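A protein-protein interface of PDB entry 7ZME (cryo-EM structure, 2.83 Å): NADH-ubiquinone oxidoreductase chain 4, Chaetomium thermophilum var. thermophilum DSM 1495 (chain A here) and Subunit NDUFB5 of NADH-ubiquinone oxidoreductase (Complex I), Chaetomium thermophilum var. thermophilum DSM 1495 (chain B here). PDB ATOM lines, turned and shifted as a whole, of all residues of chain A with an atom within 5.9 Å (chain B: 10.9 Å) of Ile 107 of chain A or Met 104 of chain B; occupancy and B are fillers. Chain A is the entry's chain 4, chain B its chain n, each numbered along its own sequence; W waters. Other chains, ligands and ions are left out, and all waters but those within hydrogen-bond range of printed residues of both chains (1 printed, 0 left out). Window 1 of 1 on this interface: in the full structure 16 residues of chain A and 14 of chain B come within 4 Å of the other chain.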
ATOM      1  N   SER A   2       7.109  29.887   8.572  1.00  0.00           N
ATOM      2  CA  SER A   2       6.675  30.205   9.922  1.00  0.00           C
ATOM      3  C   SER A   2       5.694  31.370   9.919  1.00  0.00           C
ATOM      4  O   SER A   2       5.777  32.277   9.088  1.00  0.00           O
ATOM      5  CB  SER A   2       7.872  30.545  10.808  1.00  0.00           C
ATOM      6  OG  SER A   2       7.457  30.815  12.134  1.00  0.00           O
ATOM      7  N   LEU A   4       5.758  33.596  12.035  1.00  0.00           N
ATOM      8  CA  LEU A   4       6.526  34.767  12.430  1.00  0.00           C
ATOM      9  C   LEU A   4       7.058  35.519  11.219  1.00  0.00           C
ATOM     10  O   LEU A   4       7.157  36.750  11.251  1.00  0.00           O
ATOM     11  CB  LEU A   4       7.664  34.346  13.355  1.00  0.00           C
ATOM     12  CG  LEU A   4       7.381  34.397  14.859  1.00  0.00           C
ATOM     13  CD1 LEU A   4       6.033  33.800  15.214  1.00  0.00           C
ATOM     14  CD2 LEU A   4       8.464  33.673  15.604  1.00  0.00           C
ATOM     15  N   TYR A   5       7.407  34.805  10.147  1.00  0.00           N
ATOM     16  CA  TYR A   5       7.771  35.482   8.910  1.00  0.00           C
ATOM     17  C   TYR A   5       6.545  36.023   8.193  1.00  0.00           C
ATOM     18  O   TYR A   5       6.647  37.005   7.452  1.00  0.00           O
ATOM     19  CB  TYR A   5       8.551  34.541   7.995  1.00  0.00           C
ATOM     20  CG  TYR A   5       9.840  34.033   8.586  1.00  0.00           C
ATOM     21  CD1 TYR A   5      10.935  34.870   8.736  1.00  0.00           C
ATOM     22  CD2 TYR A   5       9.967  32.716   8.990  1.00  0.00           C
ATOM     23  CE1 TYR A   5      12.117  34.406   9.272  1.00  0.00           C
ATOM     24  CE2 TYR A   5      11.144  32.244   9.525  1.00  0.00           C
ATOM     25  CZ  TYR A   5      12.216  33.090   9.665  1.00  0.00           C
ATOM     26  OH  TYR A   5      13.389  32.614  10.205  1.00  0.00           O
ATOM     27  N   PHE A 104      11.857  28.325  22.613  1.00  0.00           N
ATOM     28  CA  PHE A 104      11.167  29.318  21.747  1.00  0.00           C
ATOM     29  C   PHE A 104      10.221  28.591  20.785  1.00  0.00           C
ATOM     30  O   PHE A 104      10.575  27.506  20.306  1.00  0.00           O
ATOM     31  CB  PHE A 104      12.169  30.246  21.056  1.00  0.00           C
ATOM     32  CG  PHE A 104      12.850  31.265  21.932  1.00  0.00           C
ATOM     33  CD1 PHE A 104      12.174  32.394  22.363  1.00  0.00           C
ATOM     34  CD2 PHE A 104      14.180  31.117  22.286  1.00  0.00           C
ATOM     35  CE1 PHE A 104      12.810  33.339  23.154  1.00  0.00           C
ATOM     36  CE2 PHE A 104      14.814  32.064  23.076  1.00  0.00           C
ATOM     37  CZ  PHE A 104      14.126  33.171  23.510  1.00  0.00           C
ATOM     38  N   GLN A 105       9.054  29.171  20.496  1.00  0.00           N
ATOM     39  CA  GLN A 105       8.047  28.541  19.657  1.00  0.00           C
ATOM     40  C   GLN A 105       7.926  29.266  18.324  1.00  0.00           C
ATOM     41  O   GLN A 105       8.359  30.409  18.170  1.00  0.00           O
ATOM     42  CB  GLN A 105       6.685  28.515  20.355  1.00  0.00           C
ATOM     43  CG  GLN A 105       6.733  28.065  21.797  1.00  0.00           C
ATOM     44  CD  GLN A 105       5.448  28.353  22.539  1.00  0.00           C
ATOM     45  OE1 GLN A 105       4.375  28.403  21.945  1.00  0.00           O
ATOM     46  NE2 GLN A 105       5.548  28.539  23.846  1.00  0.00           N
ATOM     47  N   PHE A 106       7.315  28.573  17.366  1.00  0.00           N
ATOM     48  CA  PHE A 106       7.107  29.088  16.012  1.00  0.00           C
ATOM     49  C   PHE A 106       8.426  29.485  15.359  1.00  0.00           C
ATOM     50  O   PHE A 106       8.519  30.493  14.658  1.00  0.00           O
ATOM     51  CB  PHE A 106       6.104  30.241  16.009  1.00  0.00           C
ATOM     52  CG  PHE A 106       4.826  29.921  16.722  1.00  0.00           C
ATOM     53  CD1 PHE A 106       3.859  29.142  16.114  1.00  0.00           C
ATOM     54  CD2 PHE A 106       4.601  30.375  18.007  1.00  0.00           C
ATOM     55  CE1 PHE A 106       2.684  28.833  16.772  1.00  0.00           C
ATOM     56  CE2 PHE A 106       3.434  30.069  18.670  1.00  0.00           C
ATOM     57  CZ  PHE A 106       2.472  29.296  18.050  1.00  0.00           C
ATOM     58  N   ILE A 107       9.452  28.680  15.590  1.00  0.00           N
ATOM     59  CA  ILE A 107      10.731  28.842  14.922  1.00  0.00           C
ATOM     60  C   ILE A 107      10.697  28.074  13.608  1.00  0.00           C
ATOM     61  O   ILE A 107       9.883  27.171  13.408  1.00  0.00           O
ATOM     62  CB  ILE A 107      11.892  28.364  15.808  1.00  0.00           C
ATOM     63  CG1 ILE A 107      11.737  26.876  16.099  1.00  0.00           C
ATOM     64  CG2 ILE A 107      11.928  29.150  17.106  1.00  0.00           C
ATOM     65  CD1 ILE A 107      12.931  26.274  16.758  1.00  0.00           C
ATOM     66  N   GLN A 108      11.597  28.436  12.697  1.00  0.00           N
ATOM     67  CA  GLN A 108      11.683  27.791  11.394  1.00  0.00           C
ATOM     68  C   GLN A 108      13.116  27.363  11.133  1.00  0.00           C
ATOM     69  O   GLN A 108      14.046  28.155  11.322  1.00  0.00           O
ATOM     70  CB  GLN A 108      11.202  28.725  10.280  1.00  0.00           C
ATOM     71  CG  GLN A 108      11.388  28.162   8.885  1.00  0.00           C
ATOM     72  CD  GLN A 108      10.391  28.722   7.894  1.00  0.00           C
ATOM     73  OE1 GLN A 108       9.680  29.682   8.186  1.00  0.00           O
ATOM     74  NE2 GLN A 108      10.333  28.121   6.710  1.00  0.00           N
ATOM     75  N   GLU A 109      13.289  26.118  10.693  1.00  0.00           N
ATOM     76  CA  GLU A 109      14.616  25.610  10.373  1.00  0.00           C
ATOM     77  C   GLU A 109      15.232  26.403   9.230  1.00  0.00           C
ATOM     78  O   GLU A 109      14.559  26.741   8.252  1.00  0.00           O
ATOM     79  CB  GLU A 109      14.541  24.129  10.001  1.00  0.00           C
ATOM     80  CG  GLU A 109      14.315  23.200  11.178  1.00  0.00           C
ATOM     81  CD  GLU A 109      15.577  22.957  11.976  1.00  0.00           C
ATOM     82  OE1 GLU A 109      16.674  22.985  11.377  1.00  0.00           O
ATOM     83  OE2 GLU A 109      15.476  22.735  13.200  1.00  0.00           O
ATOM     84  N   ASN A 110      16.524  26.703   9.357  1.00  0.00           N
ATOM     85  CA  ASN A 110      17.245  27.432   8.320  1.00  0.00           C
ATOM     86  C   ASN A 110      18.315  26.573   7.662  1.00  0.00           C
ATOM     87  O   ASN A 110      18.273  26.380   6.443  1.00  0.00           O
ATOM     88  CB  ASN A 110      17.861  28.706   8.911  1.00  0.00           C
ATOM     89  CG  ASN A 110      18.138  29.760   7.860  1.00  0.00           C
ATOM     90  OD1 ASN A 110      17.296  30.035   7.004  1.00  0.00           O
ATOM     91  ND2 ASN A 110      19.322  30.357   7.916  1.00  0.00           N
ATOM     92  N   TYR A 119      16.761  34.947  12.663  1.00  0.00           N
ATOM     93  CA  TYR A 119      16.072  33.862  13.346  1.00  0.00           C
ATOM     94  C   TYR A 119      14.956  34.462  14.183  1.00  0.00           C
ATOM     95  O   TYR A 119      15.198  35.382  14.967  1.00  0.00           O
ATOM     96  CB  TYR A 119      17.029  33.080  14.246  1.00  0.00           C
ATOM     97  CG  TYR A 119      18.370  32.784  13.622  1.00  0.00           C
ATOM     98  CD1 TYR A 119      18.498  31.838  12.618  1.00  0.00           C
ATOM     99  CD2 TYR A 119      19.512  33.438  14.052  1.00  0.00           C
ATOM    100  CE1 TYR A 119      19.727  31.562  12.054  1.00  0.00           C
ATOM    101  CE2 TYR A 119      20.741  33.170  13.495  1.00  0.00           C
ATOM    102  CZ  TYR A 119      20.844  32.230  12.499  1.00  0.00           C
ATOM    103  OH  TYR A 119      22.070  31.958  11.939  1.00  0.00           O
ATOM    104  N   LEU A 120      13.744  33.949  14.023  1.00  0.00           N
ATOM    105  CA  LEU A 120      12.589  34.470  14.737  1.00  0.00           C
ATOM    106  C   LEU A 120      12.054  33.434  15.714  1.00  0.00           C
ATOM    107  O   LEU A 120      12.002  32.240  15.409  1.00  0.00           O
ATOM    108  CB  LEU A 120      11.476  34.894  13.773  1.00  0.00           C
ATOM    109  CG  LEU A 120      11.817  35.894  12.668  1.00  0.00           C
ATOM    110  CD1 LEU A 120      10.564  36.253  11.904  1.00  0.00           C
ATOM    111  CD2 LEU A 120      12.465  37.136  13.237  1.00  0.00           C
ATOM    112  N   GLY A 121      11.662  33.903  16.890  1.00  0.00           N
ATOM    113  CA  GLY A 121      11.058  33.047  17.891  1.00  0.00           C
ATOM    114  C   GLY A 121      10.221  33.889  18.820  1.00  0.00           C
ATOM    115  O   GLY A 121      10.355  35.114  18.862  1.00  0.00           O
ATOM    116  N   VAL A 122       9.345  33.224  19.562  1.00  0.00           N
ATOM    117  CA  VAL A 122       8.442  33.918  20.473  1.00  0.00           C
ATOM    118  C   VAL A 122       8.270  33.094  21.740  1.00  0.00           C
ATOM    119  O   VAL A 122       8.032  31.884  21.685  1.00  0.00           O
ATOM    120  CB  VAL A 122       7.085  34.229  19.806  1.00  0.00           C
ATOM    121  CG1 VAL A 122       6.298  32.969  19.519  1.00  0.00           C
ATOM    122  CG2 VAL A 122       6.283  35.188  20.664  1.00  0.00           C
ATOM    123  N   LEU A 173      15.919  36.342  17.460  1.00  0.00           N
ATOM    124  CA  LEU A 173      16.471  35.461  18.482  1.00  0.00           C
ATOM    125  C   LEU A 173      17.973  35.659  18.637  1.00  0.00           C
ATOM    126  O   LEU A 173      18.703  34.719  18.949  1.00  0.00           O
ATOM    127  CB  LEU A 173      16.161  34.003  18.155  1.00  0.00           C
ATOM    128  CG  LEU A 173      14.712  33.573  18.320  1.00  0.00           C
ATOM    129  CD1 LEU A 173      14.598  32.073  18.160  1.00  0.00           C
ATOM    130  CD2 LEU A 173      14.183  34.019  19.662  1.00  0.00           C
ATOM    131  N   TYR A 234      23.334  34.531  19.433  1.00  0.00           N
ATOM    132  CA  TYR A 234      22.112  33.740  19.421  1.00  0.00           C
ATOM    133  C   TYR A 234      21.678  33.453  20.851  1.00  0.00           C
ATOM    134  O   TYR A 234      22.499  33.113  21.705  1.00  0.00           O
ATOM    135  CB  TYR A 234      22.340  32.439  18.651  1.00  0.00           C
ATOM    136  CG  TYR A 234      21.112  31.571  18.490  1.00  0.00           C
ATOM    137  CD1 TYR A 234      20.069  31.954  17.659  1.00  0.00           C
ATOM    138  CD2 TYR A 234      21.010  30.355  19.149  1.00  0.00           C
ATOM    139  CE1 TYR A 234      18.956  31.159  17.505  1.00  0.00           C
ATOM    140  CE2 TYR A 234      19.902  29.556  18.999  1.00  0.00           C
ATOM    141  CZ  TYR A 234      18.877  29.961  18.178  1.00  0.00           C
ATOM    142  OH  TYR A 234      17.768  29.162  18.029  1.00  0.00           O
ATOM    143  N   ASP A 236      20.019  31.190  22.627  1.00  0.00           N
ATOM    144  CA  ASP A 236      20.232  29.934  23.339  1.00  0.00           C
ATOM    145  C   ASP A 236      21.685  29.771  23.760  1.00  0.00           C
ATOM    146  O   ASP A 236      21.969  29.349  24.886  1.00  0.00           O
ATOM    147  CB  ASP A 236      19.790  28.757  22.473  1.00  0.00           C
ATOM    148  CG  ASP A 236      18.285  28.673  22.331  1.00  0.00           C
ATOM    149  OD1 ASP A 236      17.576  29.356  23.101  1.00  0.00           O
ATOM    150  OD2 ASP A 236      17.810  27.922  21.453  1.00  0.00           O
ATOM    151  N   TYR B  93       2.102  20.329  19.310  1.00  0.00           N
ATOM    152  CA  TYR B  93       3.494  20.710  19.555  1.00  0.00           C
ATOM    153  C   TYR B  93       4.078  19.983  20.765  1.00  0.00           C
ATOM    154  O   TYR B  93       4.602  20.592  21.700  1.00  0.00           O
ATOM    155  CB  TYR B  93       3.610  22.222  19.712  1.00  0.00           C
ATOM    156  CG  TYR B  93       3.060  22.992  18.532  1.00  0.00           C
ATOM    157  CD1 TYR B  93       3.694  22.954  17.300  1.00  0.00           C
ATOM    158  CD2 TYR B  93       1.909  23.758  18.652  1.00  0.00           C
ATOM    159  CE1 TYR B  93       3.197  23.656  16.222  1.00  0.00           C
ATOM    160  CE2 TYR B  93       1.407  24.465  17.583  1.00  0.00           C
ATOM    161  CZ  TYR B  93       2.054  24.411  16.370  1.00  0.00           C
ATOM    162  OH  TYR B  93       1.557  25.112  15.296  1.00  0.00           O
ATOM    163  N   ASP B  95       6.725  17.811  20.968  1.00  0.00           N
ATOM    164  CA  ASP B  95       8.169  17.998  21.017  1.00  0.00           C
ATOM    165  C   ASP B  95       8.686  18.697  19.766  1.00  0.00           C
ATOM    166  O   ASP B  95       9.883  18.611  19.469  1.00  0.00           O
ATOM    167  CB  ASP B  95       8.888  16.657  21.197  1.00  0.00           C
ATOM    168  CG  ASP B  95       8.406  15.604  20.222  1.00  0.00           C
ATOM    169  OD1 ASP B  95       7.374  15.833  19.559  1.00  0.00           O
ATOM    170  OD2 ASP B  95       9.060  14.545  20.119  1.00  0.00           O
ATOM    171  N   GLU B  96       7.808  19.377  19.025  1.00  0.00           N
ATOM    172  CA  GLU B  96       8.216  20.047  17.795  1.00  0.00           C
ATOM    173  C   GLU B  96       9.299  21.080  18.064  1.00  0.00           C
ATOM    174  O   GLU B  96      10.331  21.109  17.384  1.00  0.00           O
ATOM    175  CB  GLU B  96       7.004  20.706  17.136  1.00  0.00           C
ATOM    176  CG  GLU B  96       7.292  21.306  15.773  1.00  0.00           C
ATOM    177  CD  GLU B  96       7.536  20.244  14.722  1.00  0.00           C
ATOM    178  OE1 GLU B  96       6.760  19.268  14.673  1.00  0.00           O
ATOM    179  OE2 GLU B  96       8.506  20.380  13.948  1.00  0.00           O
ATOM    180  N   TRP B  97       9.062  21.960  19.029  1.00  0.00           N
ATOM    181  CA  TRP B  97      10.006  23.091  19.202  1.00  0.00           C
ATOM    182  C   TRP B  97      11.319  22.675  19.860  1.00  0.00           C
ATOM    183  O   TRP B  97      12.335  23.242  19.485  1.00  0.00           O
ATOM    184  CB  TRP B  97       9.309  24.234  19.945  1.00  0.00           C
ATOM    185  CG  TRP B  97       8.010  24.644  19.328  1.00  0.00           C
ATOM    186  CD1 TRP B  97       6.805  24.766  19.954  1.00  0.00           C
ATOM    187  CD2 TRP B  97       7.780  24.975  17.948  1.00  0.00           C
ATOM    188  NE1 TRP B  97       5.845  25.161  19.063  1.00  0.00           N
ATOM    189  CE2 TRP B  97       6.413  25.293  17.824  1.00  0.00           C
ATOM    190  CE3 TRP B  97       8.592  25.042  16.811  1.00  0.00           C
ATOM    191  CZ2 TRP B  97       5.848  25.672  16.609  1.00  0.00           C
ATOM    192  CZ3 TRP B  97       8.031  25.409  15.610  1.00  0.00           C
ATOM    193  CH2 TRP B  97       6.676  25.714  15.514  1.00  0.00           C
ATOM    194  N   GLU B  98      11.302  21.705  20.770  1.00  0.00           N
ATOM    195  CA  GLU B  98      12.540  21.299  21.478  1.00  0.00           C
ATOM    196  C   GLU B  98      13.511  20.694  20.465  1.00  0.00           C
ATOM    197  O   GLU B  98      14.697  21.003  20.541  1.00  0.00           O
ATOM    198  CB  GLU B  98      12.210  20.322  22.600  1.00  0.00           C
ATOM    199  CG  GLU B  98      10.977  20.718  23.391  1.00  0.00           C
ATOM    200  CD  GLU B  98      11.085  20.501  24.890  1.00  0.00           C
ATOM    201  OE1 GLU B  98      11.926  19.685  25.309  1.00  0.00           O
ATOM    202  OE2 GLU B  98      10.335  21.162  25.636  1.00  0.00           O
ATOM    203  N   THR B  99      12.997  19.875  19.548  1.00  0.00           N
ATOM    204  CA  THR B  99      13.849  19.209  18.538  1.00  0.00           C
ATOM    205  C   THR B  99      14.419  20.270  17.610  1.00  0.00           C
ATOM    206  O   THR B  99      15.635  20.265  17.382  1.00  0.00           O
ATOM    207  CB  THR B  99      13.039  18.184  17.739  1.00  0.00           C
ATOM    208  OG1 THR B  99      11.837  18.807  17.286  1.00  0.00           O
ATOM    209  CG2 THR B  99      12.698  16.951  18.546  1.00  0.00           C
ATOM    210  N   ARG B 100      13.552  21.132  17.092  1.00  0.00           N
ATOM    211  CA  ARG B 100      14.012  22.189  16.199  1.00  0.00           C
ATOM    212  C   ARG B 100      14.964  23.145  16.908  1.00  0.00           C
ATOM    213  O   ARG B 100      15.994  23.528  16.347  1.00  0.00           O
ATOM    214  CB  ARG B 100      12.818  22.948  15.623  1.00  0.00           C
ATOM    215  CG  ARG B 100      11.948  22.140  14.681  1.00  0.00           C
ATOM    216  CD  ARG B 100      10.810  22.991  14.134  1.00  0.00           C
ATOM    217  NE  ARG B 100       9.898  22.223  13.291  1.00  0.00           N
ATOM    218  CZ  ARG B 100      10.050  22.058  11.981  1.00  0.00           C
ATOM    219  NH1 ARG B 100      11.082  22.608  11.357  1.00  0.00           N
ATOM    220  NH2 ARG B 100       9.170  21.344  11.294  1.00  0.00           N
ATOM    221  N   ASN B 101      14.637  23.560  18.127  1.00  0.00           N
ATOM    222  CA  ASN B 101      15.482  24.530  18.871  1.00  0.00           C
ATOM    223  C   ASN B 101      16.860  23.926  19.145  1.00  0.00           C
ATOM    224  O   ASN B 101      17.849  24.647  18.968  1.00  0.00           O
ATOM    225  CB  ASN B 101      14.832  25.004  20.176  1.00  0.00           C
ATOM    226  CG  ASN B 101      13.941  26.212  20.013  1.00  0.00           C
ATOM    227  OD1 ASN B 101      14.419  27.326  19.825  1.00  0.00           O
ATOM    228  ND2 ASN B 101      12.643  25.997  20.097  1.00  0.00           N
ATOM    229  N   THR B 102      16.915  22.675  19.602  1.00  0.00           N
ATOM    230  CA  THR B 102      18.210  22.032  19.957  1.00  0.00           C
ATOM    231  C   THR B 102      19.106  21.927  18.720  1.00  0.00           C
ATOM    232  O   THR B 102      20.319  22.132  18.863  1.00  0.00           O
ATOM    233  CB  THR B 102      18.017  20.718  20.725  1.00  0.00           C
ATOM    234  OG1 THR B 102      19.219  20.447  21.446  1.00  0.00           O
ATOM    235  CG2 THR B 102      17.680  19.531  19.848  1.00  0.00           C
ATOM    236  N   LEU B 103      18.530  21.623  17.560  1.00  0.00           N
ATOM    237  CA  LEU B 103      19.315  21.525  16.307  1.00  0.00           C
ATOM    238  C   LEU B 103      19.888  22.895  15.953  1.00  0.00           C
ATOM    239  O   LEU B 103      20.999  22.936  15.407  1.00  0.00           O
ATOM    240  CB  LEU B 103      18.400  21.021  15.191  1.00  0.00           C
ATOM    241  CG  LEU B 103      18.689  19.608  14.685  1.00  0.00           C
ATOM    242  CD1 LEU B 103      20.115  19.498  14.171  1.00  0.00           C
ATOM    243  CD2 LEU B 103      18.436  18.575  15.773  1.00  0.00           C
ATOM    244  N   MET B 104      19.156  23.967  16.251  1.00  0.00           N
ATOM    245  CA  MET B 104      19.610  25.302  15.886  1.00  0.00           C
ATOM    246  C   MET B 104      20.755  25.754  16.777  1.00  0.00           C
ATOM    247  O   MET B 104      21.713  26.372  16.302  1.00  0.00           O
ATOM    248  CB  MET B 104      18.450  26.283  15.979  1.00  0.00           C
ATOM    249  CG  MET B 104      17.379  26.029  14.955  1.00  0.00           C
ATOM    250  SD  MET B 104      16.008  27.181  15.077  1.00  0.00           S
ATOM    251  CE  MET B 104      14.948  26.504  13.817  1.00  0.00           C
ATOM    252  N   ALA B 105      20.669  25.467  18.076  1.00  0.00           N
ATOM    253  CA  ALA B 105      21.735  25.859  18.985  1.00  0.00           C
ATOM    254  C   ALA B 105      23.030  25.136  18.650  1.00  0.00           C
ATOM    255  O   ALA B 105      24.102  25.752  18.623  1.00  0.00           O
ATOM    256  CB  ALA B 105      21.320  25.592  20.429  1.00  0.00           C
ATOM    257  N   ALA B 106      22.949  23.836  18.366  1.00  0.00           N
ATOM    258  CA  ALA B 106      24.139  23.081  17.991  1.00  0.00           C
ATOM    259  C   ALA B 106      24.763  23.627  16.715  1.00  0.00           C
ATOM    260  O   ALA B 106      25.989  23.739  16.611  1.00  0.00           O
ATOM    261  CB  ALA B 106      23.791  21.603  17.826  1.00  0.00           C
ATOM    262  N   ALA B 107      23.934  23.971  15.731  1.00  0.00           N
ATOM    263  CA  ALA B 107      24.451  24.498  14.474  1.00  0.00           C
ATOM    264  C   ALA B 107      25.193  25.807  14.689  1.00  0.00           C
ATOM    265  O   ALA B 107      26.183  26.089  14.006  1.00  0.00           O
ATOM    266  CB  ALA B 107      23.309  24.680  13.475  1.00  0.00           C
ATOM    267  N   LEU B 108      24.736  26.617  15.639  1.00  0.00           N
ATOM    268  CA  LEU B 108      25.386  27.881  15.951  1.00  0.00           C
ATOM    269  C   LEU B 108      26.469  27.756  17.013  1.00  0.00           C
ATOM    270  O   LEU B 108      27.342  28.625  17.083  1.00  0.00           O
ATOM    271  CB  LEU B 108      24.334  28.908  16.376  1.00  0.00           C
ATOM    272  CG  LEU B 108      23.362  29.185  15.228  1.00  0.00           C
ATOM    273  CD1 LEU B 108      22.114  29.872  15.703  1.00  0.00           C
ATOM    274  CD2 LEU B 108      24.052  30.020  14.169  1.00  0.00           C
ATOM    275  N   GLU B 109      26.433  26.711  17.846  1.00  0.00           N
ATOM    276  CA  GLU B 109      27.617  26.344  18.616  1.00  0.00           C
ATOM    277  C   GLU B 109      28.790  26.042  17.695  1.00  0.00           C
ATOM    278  O   GLU B 109      29.899  26.550  17.890  1.00  0.00           O
ATOM    279  CB  GLU B 109      27.336  25.125  19.499  1.00  0.00           C
ATOM    280  CG  GLU B 109      26.344  25.288  20.634  1.00  0.00           C
ATOM    281  CD  GLU B 109      26.835  26.224  21.717  1.00  0.00           C
ATOM    282  OE1 GLU B 109      28.063  26.287  21.941  1.00  0.00           O
ATOM    283  OE2 GLU B 109      25.992  26.851  22.384  1.00  0.00           O
ATOM    284  N   GLN B 110      28.560  25.198  16.688  1.00  0.00           N
ATOM    285  CA  GLN B 110      29.643  24.779  15.806  1.00  0.00           C
ATOM    286  C   GLN B 110      30.167  25.945  14.982  1.00  0.00           C
ATOM    287  O   GLN B 110      31.377  26.059  14.759  1.00  0.00           O
ATOM    288  CB  GLN B 110      29.171  23.644  14.899  1.00  0.00           C
ATOM    289  CG  GLN B 110      28.793  22.383  15.650  1.00  0.00           C
ATOM    290  CD  GLN B 110      29.982  21.733  16.331  1.00  0.00           C
ATOM    291  OE1 GLN B 110      31.084  21.700  15.783  1.00  0.00           O
ATOM    292  NE2 GLN B 110      29.763  21.215  17.533  1.00  0.00           N
ATOM    293  N   ALA B 111      29.251  26.817  14.559  1.00  0.00           N
ATOM    294  CA  ALA B 111      29.628  28.063  13.860  1.00  0.00           C
ATOM    295  C   ALA B 111      30.632  28.815  14.728  1.00  0.00           C
ATOM    296  O   ALA B 111      31.685  29.207  14.208  1.00  0.00           O
ATOM    297  CB  ALA B 111      28.402  28.891  13.605  1.00  0.00           C
ATOM    298  N   ALA B 112      30.291  29.022  16.002  1.00  0.00           N
ATOM    299  CA  ALA B 112      31.136  29.823  16.917  1.00  0.00           C
ATOM    300  C   ALA B 112      32.516  29.187  17.100  1.00  0.00           C
ATOM    301  O   ALA B 112      33.499  29.937  17.141  1.00  0.00           O
ATOM    302  CB  ALA B 112      30.432  30.001  18.235  1.00  0.00           C
HETATM  303  O   HOH W   1       3.134  25.969  20.927  1.00  0.00           O
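Of chain B, only Trp 97 (3.4 Å), Arg 100 (3.5 Å), Asn 101 (3.4 Å) and Met 104 (3.6 Å) come within 4 Å of Ile 107 of chain A.
Printed residues of chain B within 4 Å of Tyr 234 of chain A: Met 104 (3.6 Å) and Leu 108 (3.4 Å).
Of the printed residues of chain A, Asn 101 of chain B touches Phe 104 (2.6 Å), Ile 107 (3.4 Å) and Asp 236 (3.8 Å).
Of the printed residues of chain B, Asp 236 of chain A touches Asn 101 (3.8 Å).
Of the printed residues of chain B, Phe 104 of chain A touches Trp 97 and Asn 101.
Of the printed residues of chain B, Tyr 119 of chain A touches Leu 108 (3.6 Å).
Val 122 of chain A touches none of the printed residues of chain B.
The nearest residue of chain B that does not touch Ile 107 of chain A is Glu 96 of chain B (5.8 Å).
Phe 104 of chain A touches Trp 97 of chain B (O to CB, 3.5 Å).
Trp 97 of chain B touches Gln 105 of chain A (NE1 to CB, 3.7 Å).
Trp 97 of chain B touches Ile 107 of chain A (CZ3 to O, 3.4 Å).
Ile 107 of chain A touches Asn 101 of chain B.
Met 104 of chain B touches Ile 107 of chain A.
Gln 108 of chain A touches Met 104 of chain B.
OE2 of Glu 109 of chain A touches CB of Leu 103 of chain B, at 3.9 Å.
Glu 109 of chain A touches Met 104 of chain B (N to CE, 3.6 Å).
OH of Tyr 119 of chain A touches CD2 of Leu 108 of chain B, at 3.6 Å.
OD2 of Asp 236 of chain A touches OD1 of Asn 101 of chain B (3.8 Å).
Of the 19 printed residues of chain B, 6 touch a printed residue of chain A.
Printed residues of chain B that touch a printed residue of chain A: Trp 97, Arg 100, Asn 101, Leu 103, Met 104 and Leu 108.
Hydrophobic or aromatic side chains of chain B within 4 Å of the printed part of chain A: Trp 97, Leu 103, Met 104 and Leu 108.
Along chain B the printed residues that touch a printed residue of chain A span positions 97 to 108.
Of the 17 printed residues of chain A, 9 touch a printed residue of chain B.
Hydrophobic or aromatic side chains of chain A that line the printed part of chain B: Phe 104, Ile 107, Tyr 119 and Tyr 234.
Among the printed residues, no Asp or Glu carboxylate lies within 4 Å of a Lys or Arg side-chain nitrogen of the other chain.
ND2 of Asn 101 of chain B is in hydrogen-bond range of O of Phe 104 of chain A, at 2.6 Å.
The backbone carbonyl oxygen (O) of Arg 100 of chain B sits close to the side-chain carboxylate (OE2) of Glu 109 of chain A, at 3.3 Å.
Water W1 bridges the side-chain amide oxygen (OE1) of Gln 105 of chain A (2.9 Å) and the indole nitrogen (NE1) of Trp 97 of chain B (3.4 Å).
OE2 of Glu 96 of chain B is in salt-bridge range of NE of Arg 100 of chain B (2.4 Å).
ND2 of Asn 101 of chain B sits at hydrogen-bond distance from O of Trp 97 of chain B (2.8 Å).
The side-chain hydroxyl (OG) of Ser 2 of chain A sits at hydrogen-bond distance from the backbone carbonyl oxygen (O) of Phe 106 of chain A (2.8 Å).
N of Ser 2 of chain A sits at hydrogen-bond distance from OE1 of Gln 108 of chain A (2.6 Å).
N of Gln 105 of chain A lies within hydrogen-bond range of O of Val 122 of chain A (3.1 Å).
The backbone NH of Leu 173 of chain A sits at hydrogen-bond distance from the backbone carbonyl oxygen of Tyr 119 of chain A (2.8 Å).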
